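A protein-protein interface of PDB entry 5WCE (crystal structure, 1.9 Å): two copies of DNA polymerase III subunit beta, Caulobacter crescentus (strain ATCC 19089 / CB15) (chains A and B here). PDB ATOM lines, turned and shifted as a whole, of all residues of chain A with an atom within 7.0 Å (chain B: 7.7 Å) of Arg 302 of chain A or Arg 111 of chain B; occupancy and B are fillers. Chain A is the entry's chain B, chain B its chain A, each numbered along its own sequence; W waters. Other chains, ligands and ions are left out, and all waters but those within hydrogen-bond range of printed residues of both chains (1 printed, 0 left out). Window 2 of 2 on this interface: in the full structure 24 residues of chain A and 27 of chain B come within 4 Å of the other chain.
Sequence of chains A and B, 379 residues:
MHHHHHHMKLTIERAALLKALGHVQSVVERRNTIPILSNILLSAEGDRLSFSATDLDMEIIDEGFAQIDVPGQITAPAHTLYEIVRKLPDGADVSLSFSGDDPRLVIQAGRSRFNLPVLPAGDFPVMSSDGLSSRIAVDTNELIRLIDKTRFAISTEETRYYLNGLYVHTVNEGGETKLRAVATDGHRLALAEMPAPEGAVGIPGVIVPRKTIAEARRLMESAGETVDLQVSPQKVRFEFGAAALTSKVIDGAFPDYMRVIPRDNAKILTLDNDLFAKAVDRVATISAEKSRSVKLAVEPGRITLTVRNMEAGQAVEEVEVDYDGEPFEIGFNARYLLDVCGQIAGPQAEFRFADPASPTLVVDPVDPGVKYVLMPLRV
The backbone NH (N) of Arg 113 of chain B sits at hydrogen-bond distance from the backbone carbonyl oxygen (O) of Val 316 of chain A.
NH1 of Arg 111 of chain B lies within salt-bridge range of OE1 of Glu 318 of chain A (2.7 Å).
The side-chain hydroxyl (OG) of Ser 112 of chain B sits at hydrogen-bond distance from the side-chain carboxylate (OE1) of Glu 317 of chain A, 2.8 Å away.
NH2 of Arg 111 of chain B lies within salt-bridge range of OE2 of Glu 320 of chain A, 3.7 Å away.
OG of Ser 112 of chain B lies within hydrogen-bond range of NE of Arg 282 of chain A.
NE of Arg 282 of chain A is in salt-bridge range of OE1 of Glu 317 of chain A (2.8 Å).
The side-chain carboxylate (OE1) of Glu 318 of chain A lies within salt-bridge range of the guanidinium group (NH1) of Arg 302 of chain A (3.6 Å).
The guanidinium group (NH1) of Arg 113 of chain B sits at hydrogen-bond distance from the side-chain amide oxygen (OE1) of Gln 108 of chain B (2.8 Å).
Among the printed residues, pairs that only touch across the chains: Arg 282 of chain A with Leu 88 of chain B, Arg 282 of chain A with Phe 114 of chain B, Arg 302 of chain A with Arg 111 of chain B, Val 316 of chain A with Arg 111 of chain B, Val 316 of chain A with Ser 112 of chain B and Glu 317 of chain A with Arg 111 of chain B.
Of chain B, only Arg 111 (3.5 Å) comes within 4 Å of Arg 302 of chain A.
Printed residues of chain A within 4 Å of Arg 111 of chain B: Arg 302 (3.5 Å), Val 316 (3.9 Å), Glu 317 (3.4 Å), Glu 318 (2.7 Å) and Glu 320 (3.1 Å).
No residue of chain B comes within 4 Å of Gly 301 of chain A.
Of the printed residues of chain A, Leu 88 of chain B touches Arg 282 (3.9 Å).
Of the printed residues of chain B, Glu 318 of chain A touches Arg 111.
Of the printed residues of chain A, Ser 112 of chain B touches Arg 282, Val 316 and Glu 317.
Val 321 of chain A touches none of the printed residues of chain B.
Ala 297 of chain A touches none of the printed residues of chain B.
Of the 18 printed residues of chain A, 6 touch a printed residue of chain B.
Printed residues of chain B that touch a printed residue of chain A: Leu 88, Arg 111, Ser 112, Arg 113 and Phe 114.
Hydrophobic or aromatic side chains of chain B that line the printed part of chain A: Leu 88 and Phe 114.
Among the printed residues, 11 pairs touch across the chains.
Among the printed residues, Asp or Glu carboxylates within 4 Å of a Lys or Arg side-chain nitrogen of the other chain: Glu 318 of chain A with Arg 111 of chain B (2.7 Å) and Glu 320 of chain A with Arg 111 of chain B (3.7 Å).
No position is printed for both chains.
Of the 11 pairs that touch across the chains among the printed residues, none has its exchanged pair printed and touching as well.
Water W1 bridges OE1 of Glu 318 of chain A (2.8 Å) and NH1 of Arg 111 of chain B (3.2 Å).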
ATOM      1  N   LEU A 269      32.737 -31.213   2.428  1.00  0.00           N
ATOM      2  CA  LEU A 269      31.920 -30.070   2.653  1.00  0.00           C
ATOM      3  C   LEU A 269      31.255 -30.199   4.023  1.00  0.00           C
ATOM      4  O   LEU A 269      30.751 -31.248   4.339  1.00  0.00           O
ATOM      5  CB  LEU A 269      30.881 -30.087   1.500  1.00  0.00           C
ATOM      6  CG  LEU A 269      29.752 -29.138   1.356  1.00  0.00           C
ATOM      7  CD1 LEU A 269      29.353 -29.145  -0.107  1.00  0.00           C
ATOM      8  CD2 LEU A 269      28.607 -29.472   2.342  1.00  0.00           C
ATOM      9  N   ARG A 282      11.826 -27.145   2.294  1.00  0.00           N
ATOM     10  CA  ARG A 282      11.178 -26.083   1.554  1.00  0.00           C
ATOM     11  C   ARG A 282      11.072 -26.336   0.031  1.00  0.00           C
ATOM     12  O   ARG A 282       9.971 -26.364  -0.550  1.00  0.00           O
ATOM     13  CB  ARG A 282      11.841 -24.714   1.795  1.00  0.00           C
ATOM     14  CG  ARG A 282      11.306 -23.977   2.995  1.00  0.00           C
ATOM     15  CD  ARG A 282      11.823 -22.590   3.047  1.00  0.00           C
ATOM     16  NE  ARG A 282      13.239 -22.546   3.409  1.00  0.00           N
ATOM     17  CZ  ARG A 282      13.709 -22.608   4.650  1.00  0.00           C
ATOM     18  NH1 ARG A 282      12.913 -22.709   5.702  1.00  0.00           N
ATOM     19  NH2 ARG A 282      15.029 -22.574   4.841  1.00  0.00           N
ATOM     20  N   ALA A 297      23.554 -27.737  -6.526  1.00  0.00           N
ATOM     21  CA  ALA A 297      24.625 -27.088  -7.276  1.00  0.00           C
ATOM     22  C   ALA A 297      25.651 -26.596  -6.274  1.00  0.00           C
ATOM     23  O   ALA A 297      25.399 -25.640  -5.558  1.00  0.00           O
ATOM     24  CB  ALA A 297      24.077 -25.968  -8.159  1.00  0.00           C
ATOM     25  N   VAL A 298      26.767 -27.327  -6.176  1.00  0.00           N
ATOM     26  CA  VAL A 298      27.797 -27.118  -5.152  1.00  0.00           C
ATOM     27  C   VAL A 298      28.914 -26.290  -5.752  1.00  0.00           C
ATOM     28  O   VAL A 298      29.392 -26.572  -6.863  1.00  0.00           O
ATOM     29  CB  VAL A 298      28.326 -28.481  -4.613  1.00  0.00           C
ATOM     30  CG1 VAL A 298      29.353 -28.298  -3.519  1.00  0.00           C
ATOM     31  CG2 VAL A 298      27.165 -29.364  -4.154  1.00  0.00           C
ATOM     32  N   GLU A 299      29.287 -25.240  -5.043  1.00  0.00           N
ATOM     33  CA  GLU A 299      30.447 -24.411  -5.419  1.00  0.00           C
ATOM     34  C   GLU A 299      31.085 -23.879  -4.153  1.00  0.00           C
ATOM     35  O   GLU A 299      30.487 -23.972  -3.096  1.00  0.00           O
ATOM     36  CB  GLU A 299      29.983 -23.244  -6.326  1.00  0.00           C
ATOM     37  CG  GLU A 299      29.020 -22.278  -5.632  1.00  0.00           C
ATOM     38  CD  GLU A 299      28.464 -21.205  -6.603  1.00  0.00           C
ATOM     39  OE1 GLU A 299      29.235 -20.414  -7.137  1.00  0.00           O
ATOM     40  OE2 GLU A 299      27.248 -21.165  -6.809  1.00  0.00           O
ATOM     41  N   PRO A 300      32.300 -23.275  -4.253  1.00  0.00           N
ATOM     42  CA  PRO A 300      32.853 -22.671  -3.055  1.00  0.00           C
ATOM     43  C   PRO A 300      31.863 -21.793  -2.312  1.00  0.00           C
ATOM     44  O   PRO A 300      31.177 -20.971  -2.924  1.00  0.00           O
ATOM     45  CB  PRO A 300      34.077 -21.882  -3.579  1.00  0.00           C
ATOM     46  CG  PRO A 300      34.542 -22.724  -4.686  1.00  0.00           C
ATOM     47  CD  PRO A 300      33.291 -23.272  -5.344  1.00  0.00           C
ATOM     48  N   GLY A 301      31.740 -22.027  -1.020  1.00  0.00           N
ATOM     49  CA  GLY A 301      30.802 -21.275  -0.192  1.00  0.00           C
ATOM     50  C   GLY A 301      29.296 -21.556  -0.216  1.00  0.00           C
ATOM     51  O   GLY A 301      28.552 -21.015   0.618  1.00  0.00           O
ATOM     52  N   ARG A 302      28.807 -22.386  -1.132  1.00  0.00           N
ATOM     53  CA  ARG A 302      27.365 -22.426  -1.367  1.00  0.00           C
ATOM     54  C   ARG A 302      26.852 -23.695  -2.029  1.00  0.00           C
ATOM     55  O   ARG A 302      27.472 -24.261  -2.920  1.00  0.00           O
ATOM     56  CB  ARG A 302      27.019 -21.175  -2.225  1.00  0.00           C
ATOM     57  CG  ARG A 302      25.641 -21.076  -2.756  1.00  0.00           C
ATOM     58  CD  ARG A 302      25.483 -19.814  -3.626  1.00  0.00           C
ATOM     59  NE  ARG A 302      25.601 -18.609  -2.817  1.00  0.00           N
ATOM     60  CZ  ARG A 302      25.554 -17.378  -3.301  1.00  0.00           C
ATOM     61  NH1 ARG A 302      25.344 -17.187  -4.609  1.00  0.00           N
ATOM     62  NH2 ARG A 302      25.694 -16.334  -2.478  1.00  0.00           N
ATOM     63  N   ILE A 303      25.677 -24.102  -1.610  1.00  0.00           N
ATOM     64  CA  ILE A 303      24.859 -25.049  -2.368  1.00  0.00           C
ATOM     65  C   ILE A 303      23.603 -24.338  -2.775  1.00  0.00           C
ATOM     66  O   ILE A 303      22.936 -23.740  -1.948  1.00  0.00           O
ATOM     67  CB  ILE A 303      24.490 -26.301  -1.557  1.00  0.00           C
ATOM     68  CG1 ILE A 303      25.755 -27.033  -1.148  1.00  0.00           C
ATOM     69  CG2 ILE A 303      23.535 -27.210  -2.351  1.00  0.00           C
ATOM     70  CD1 ILE A 303      25.469 -28.262  -0.293  1.00  0.00           C
ATOM     71  N   THR A 304      23.299 -24.385  -4.065  1.00  0.00           N
ATOM     72  CA  THR A 304      22.020 -23.895  -4.573  1.00  0.00           C
ATOM     73  C   THR A 304      21.133 -25.110  -4.778  1.00  0.00           C
ATOM     74  O   THR A 304      21.481 -25.991  -5.547  1.00  0.00           O
ATOM     75  CB  THR A 304      22.209 -23.055  -5.851  1.00  0.00           C
ATOM     76  OG1 THR A 304      23.089 -21.975  -5.548  1.00  0.00           O
ATOM     77  CG2 THR A 304      20.901 -22.463  -6.317  1.00  0.00           C
ATOM     78  N   VAL A 316      13.830 -22.738  -5.685  1.00  0.00           N
ATOM     79  CA  VAL A 316      15.253 -22.565  -5.490  1.00  0.00           C
ATOM     80  C   VAL A 316      15.562 -21.973  -4.116  1.00  0.00           C
ATOM     81  O   VAL A 316      14.955 -20.961  -3.715  1.00  0.00           O
ATOM     82  CB  VAL A 316      15.839 -21.631  -6.530  1.00  0.00           C
ATOM     83  CG1 VAL A 316      17.349 -21.493  -6.423  1.00  0.00           C
ATOM     84  CG2 VAL A 316      15.455 -22.155  -7.905  1.00  0.00           C
ATOM     85  N   GLU A 317      16.581 -22.524  -3.445  1.00  0.00           N
ATOM     86  CA  GLU A 317      17.167 -21.879  -2.265  1.00  0.00           C
ATOM     87  C   GLU A 317      18.690 -21.998  -2.216  1.00  0.00           C
ATOM     88  O   GLU A 317      19.214 -23.079  -2.477  1.00  0.00           O
ATOM     89  CB  GLU A 317      16.534 -22.472  -1.002  1.00  0.00           C
ATOM     90  CG  GLU A 317      17.043 -21.810   0.277  1.00  0.00           C
ATOM     91  CD  GLU A 317      16.114 -21.988   1.450  1.00  0.00           C
ATOM     92  OE1 GLU A 317      14.973 -22.482   1.272  1.00  0.00           O
ATOM     93  OE2 GLU A 317      16.553 -21.671   2.579  1.00  0.00           O
ATOM     94  N   GLU A 318      19.369 -20.901  -1.885  1.00  0.00           N
ATOM     95  CA  GLU A 318      20.806 -20.901  -1.641  1.00  0.00           C
ATOM     96  C   GLU A 318      21.093 -21.098  -0.164  1.00  0.00           C
ATOM     97  O   GLU A 318      20.444 -20.498   0.702  1.00  0.00           O
ATOM     98  CB  GLU A 318      21.436 -19.587  -2.088  1.00  0.00           C
ATOM     99  CG  GLU A 318      21.229 -19.353  -3.567  1.00  0.00           C
ATOM    100  CD  GLU A 318      21.660 -17.968  -4.048  1.00  0.00           C
ATOM    101  OE1 GLU A 318      22.007 -17.085  -3.231  1.00  0.00           O
ATOM    102  OE2 GLU A 318      21.688 -17.771  -5.273  1.00  0.00           O
ATOM    103  N   VAL A 319      22.051 -21.989   0.114  1.00  0.00           N
ATOM    104  CA  VAL A 319      22.476 -22.300   1.479  1.00  0.00           C
ATOM    105  C   VAL A 319      23.998 -22.136   1.526  1.00  0.00           C
ATOM    106  O   VAL A 319      24.720 -22.705   0.703  1.00  0.00           O
ATOM    107  CB  VAL A 319      22.084 -23.712   1.908  1.00  0.00           C
ATOM    108  CG1 VAL A 319      22.629 -24.015   3.291  1.00  0.00           C
ATOM    109  CG2 VAL A 319      20.565 -23.858   1.899  1.00  0.00           C
ATOM    110  N   GLU A 320      24.460 -21.334   2.466  1.00  0.00           N
ATOM    111  CA  GLU A 320      25.888 -21.133   2.673  1.00  0.00           C
ATOM    112  C   GLU A 320      26.494 -22.429   3.295  1.00  0.00           C
ATOM    113  O   GLU A 320      25.913 -23.048   4.133  1.00  0.00           O
ATOM    114  CB  GLU A 320      26.158 -19.889   3.545  1.00  0.00           C
ATOM    115  CG  GLU A 320      25.422 -18.635   3.041  1.00  0.00           C
ATOM    116  CD  GLU A 320      25.608 -17.409   3.924  1.00  0.00           C
ATOM    117  OE1 GLU A 320      26.010 -17.504   5.100  1.00  0.00           O
ATOM    118  OE2 GLU A 320      25.374 -16.326   3.414  1.00  0.00           O
ATOM    119  N   VAL A 321      27.633 -22.861   2.770  1.00  0.00           N
ATOM    120  CA  VAL A 321      28.310 -24.057   3.282  1.00  0.00           C
ATOM    121  C   VAL A 321      29.805 -23.803   3.270  1.00  0.00           C
ATOM    122  O   VAL A 321      30.265 -22.861   2.679  1.00  0.00           O
ATOM    123  CB  VAL A 321      27.997 -25.352   2.464  1.00  0.00           C
ATOM    124  CG1 VAL A 321      26.474 -25.593   2.352  1.00  0.00           C
ATOM    125  CG2 VAL A 321      28.632 -25.303   1.077  1.00  0.00           C
ATOM    126  N   ASP A 322      30.530 -24.651   3.997  1.00  0.00           N
ATOM    127  CA  ASP A 322      31.983 -24.638   4.074  1.00  0.00           C
ATOM    128  C   ASP A 322      32.558 -25.611   3.046  1.00  0.00           C
ATOM    129  O   ASP A 322      32.598 -26.854   3.281  1.00  0.00           O
ATOM    130  CB  ASP A 322      32.395 -25.068   5.483  1.00  0.00           C
ATOM    131  CG  ASP A 322      33.846 -24.774   5.800  1.00  0.00           C
ATOM    132  OD1 ASP A 322      34.600 -24.187   4.952  1.00  0.00           O
ATOM    133  OD2 ASP A 322      34.212 -25.102   6.954  1.00  0.00           O
ATOM    134  N   TYR A 323      33.044 -25.047   1.939  1.00  0.00           N
ATOM    135  CA  TYR A 323      33.623 -25.805   0.823  1.00  0.00           C
ATOM    136  C   TYR A 323      34.505 -24.940  -0.047  1.00  0.00           C
ATOM    137  O   TYR A 323      34.121 -23.815  -0.369  1.00  0.00           O
ATOM    138  CB  TYR A 323      32.454 -26.374  -0.023  1.00  0.00           C
ATOM    139  CG  TYR A 323      32.876 -27.179  -1.202  1.00  0.00           C
ATOM    140  CD1 TYR A 323      33.520 -28.386  -1.036  1.00  0.00           C
ATOM    141  CD2 TYR A 323      32.623 -26.760  -2.491  1.00  0.00           C
ATOM    142  CE1 TYR A 323      33.909 -29.161  -2.121  1.00  0.00           C
ATOM    143  CE2 TYR A 323      33.040 -27.510  -3.592  1.00  0.00           C
ATOM    144  CZ  TYR A 323      33.676 -28.734  -3.398  1.00  0.00           C
ATOM    145  OH  TYR A 323      34.092 -29.522  -4.486  1.00  0.00           O
ATOM    146  N   LEU B  88       8.511 -21.606   5.691  1.00  0.00           N
ATOM    147  CA  LEU B  88       9.363 -20.432   5.703  1.00  0.00           C
ATOM    148  C   LEU B  88       9.807 -20.090   7.132  1.00  0.00           C
ATOM    149  O   LEU B  88       9.125 -20.406   8.072  1.00  0.00           O
ATOM    150  CB  LEU B  88       8.680 -19.229   5.027  1.00  0.00           C
ATOM    151  CG  LEU B  88       8.380 -19.314   3.527  1.00  0.00           C
ATOM    152  CD1 LEU B  88       7.498 -18.182   3.023  1.00  0.00           C
ATOM    153  CD2 LEU B  88       9.673 -19.377   2.755  1.00  0.00           C
ATOM    154  N   PRO B  89      10.986 -19.459   7.296  1.00  0.00           N
ATOM    155  CA  PRO B  89      11.432 -19.133   8.676  1.00  0.00           C
ATOM    156  C   PRO B  89      10.430 -18.245   9.422  1.00  0.00           C
ATOM    157  O   PRO B  89       9.802 -17.383   8.806  1.00  0.00           O
ATOM    158  CB  PRO B  89      12.719 -18.375   8.475  1.00  0.00           C
ATOM    159  CG  PRO B  89      13.039 -18.439   7.033  1.00  0.00           C
ATOM    160  CD  PRO B  89      11.825 -18.827   6.283  1.00  0.00           C
ATOM    161  N   GLN B 108       8.780 -15.054  -2.712  1.00  0.00           N
ATOM    162  CA  GLN B 108      10.146 -14.902  -2.254  1.00  0.00           C
ATOM    163  C   GLN B 108      10.182 -14.497  -0.791  1.00  0.00           C
ATOM    164  O   GLN B 108       9.421 -13.623  -0.345  1.00  0.00           O
ATOM    165  CB  GLN B 108      10.809 -13.857  -3.091  1.00  0.00           C
ATOM    166  CG  GLN B 108      12.222 -13.594  -2.614  1.00  0.00           C
ATOM    167  CD  GLN B 108      13.153 -13.496  -3.773  1.00  0.00           C
ATOM    168  OE1 GLN B 108      12.811 -12.872  -4.798  1.00  0.00           O
ATOM    169  NE2 GLN B 108      14.316 -14.146  -3.658  1.00  0.00           N
ATOM    170  N   ALA B 109      11.104 -15.104  -0.066  1.00  0.00           N
ATOM    171  CA  ALA B 109      11.322 -14.836   1.340  1.00  0.00           C
ATOM    172  C   ALA B 109      12.681 -15.348   1.740  1.00  0.00           C
ATOM    173  O   ALA B 109      12.975 -16.525   1.553  1.00  0.00           O
ATOM    174  CB  ALA B 109      10.288 -15.548   2.172  1.00  0.00           C
ATOM    175  N   GLY B 110      13.497 -14.442   2.277  1.00  0.00           N
ATOM    176  CA  GLY B 110      14.865 -14.748   2.694  1.00  0.00           C
ATOM    177  C   GLY B 110      15.596 -15.154   1.455  1.00  0.00           C
ATOM    178  O   GLY B 110      15.566 -14.466   0.474  1.00  0.00           O
ATOM    179  N   ARG B 111      16.167 -16.345   1.481  1.00  0.00           N
ATOM    180  CA  ARG B 111      16.954 -16.845   0.352  1.00  0.00           C
ATOM    181  C   ARG B 111      16.196 -17.933  -0.457  1.00  0.00           C
ATOM    182  O   ARG B 111      16.829 -18.687  -1.202  1.00  0.00           O
ATOM    183  CB  ARG B 111      18.294 -17.383   0.932  1.00  0.00           C
ATOM    184  CG  ARG B 111      19.083 -16.297   1.690  1.00  0.00           C
ATOM    185  CD  ARG B 111      20.288 -15.804   0.908  1.00  0.00           C
ATOM    186  NE  ARG B 111      21.335 -16.748   1.234  1.00  0.00           N
ATOM    187  CZ  ARG B 111      22.389 -17.091   0.515  1.00  0.00           C
ATOM    188  NH1 ARG B 111      22.707 -16.535  -0.650  1.00  0.00           N
ATOM    189  NH2 ARG B 111      23.156 -18.034   1.024  1.00  0.00           N
ATOM    190  N   SER B 112      14.886 -18.048  -0.240  1.00  0.00           N
ATOM    191  CA  SER B 112      13.994 -18.933  -1.010  1.00  0.00           C
ATOM    192  C   SER B 112      13.181 -18.188  -2.068  1.00  0.00           C
ATOM    193  O   SER B 112      12.634 -17.094  -1.790  1.00  0.00           O
ATOM    194  CB  SER B 112      12.918 -19.578  -0.101  1.00  0.00           C
ATOM    195  OG  SER B 112      13.460 -20.130   1.061  1.00  0.00           O
ATOM    196  N   ARG B 113      13.041 -18.808  -3.239  1.00  0.00           N
ATOM    197  CA  ARG B 113      12.200 -18.296  -4.323  1.00  0.00           C
ATOM    198  C   ARG B 113      11.411 -19.438  -4.942  1.00  0.00           C
ATOM    199  O   ARG B 113      12.010 -20.462  -5.352  1.00  0.00           O
ATOM    200  CB  ARG B 113      13.058 -17.636  -5.381  1.00  0.00           C
ATOM    201  CG  ARG B 113      12.282 -16.915  -6.479  1.00  0.00           C
ATOM    202  CD  ARG B 113      13.284 -16.432  -7.511  1.00  0.00           C
ATOM    203  NE  ARG B 113      12.695 -15.693  -8.592  1.00  0.00           N
ATOM    204  CZ  ARG B 113      12.334 -14.411  -8.542  1.00  0.00           C
ATOM    205  NH1 ARG B 113      12.426 -13.707  -7.403  1.00  0.00           N
ATOM    206  NH2 ARG B 113      11.806 -13.826  -9.627  1.00  0.00           N
ATOM    207  N   PHE B 114      10.079 -19.288  -4.996  1.00  0.00           N
ATOM    208  CA  PHE B 114       9.228 -20.259  -5.634  1.00  0.00           C
ATOM    209  C   PHE B 114       8.482 -19.612  -6.811  1.00  0.00           C
ATOM    210  O   PHE B 114       8.098 -18.444  -6.739  1.00  0.00           O
ATOM    211  CB  PHE B 114       8.230 -20.827  -4.665  1.00  0.00           C
ATOM    212  CG  PHE B 114       8.837 -21.396  -3.422  1.00  0.00           C
ATOM    213  CD1 PHE B 114       9.280 -20.558  -2.396  1.00  0.00           C
ATOM    214  CD2 PHE B 114       8.953 -22.757  -3.266  1.00  0.00           C
ATOM    215  CE1 PHE B 114       9.884 -21.072  -1.261  1.00  0.00           C
ATOM    216  CE2 PHE B 114       9.539 -23.290  -2.116  1.00  0.00           C
ATOM    217  CZ  PHE B 114      10.007 -22.442  -1.118  1.00  0.00           C
HETATM  218  O   HOH W   1      21.903 -14.338  -2.841  1.00  0.00           O
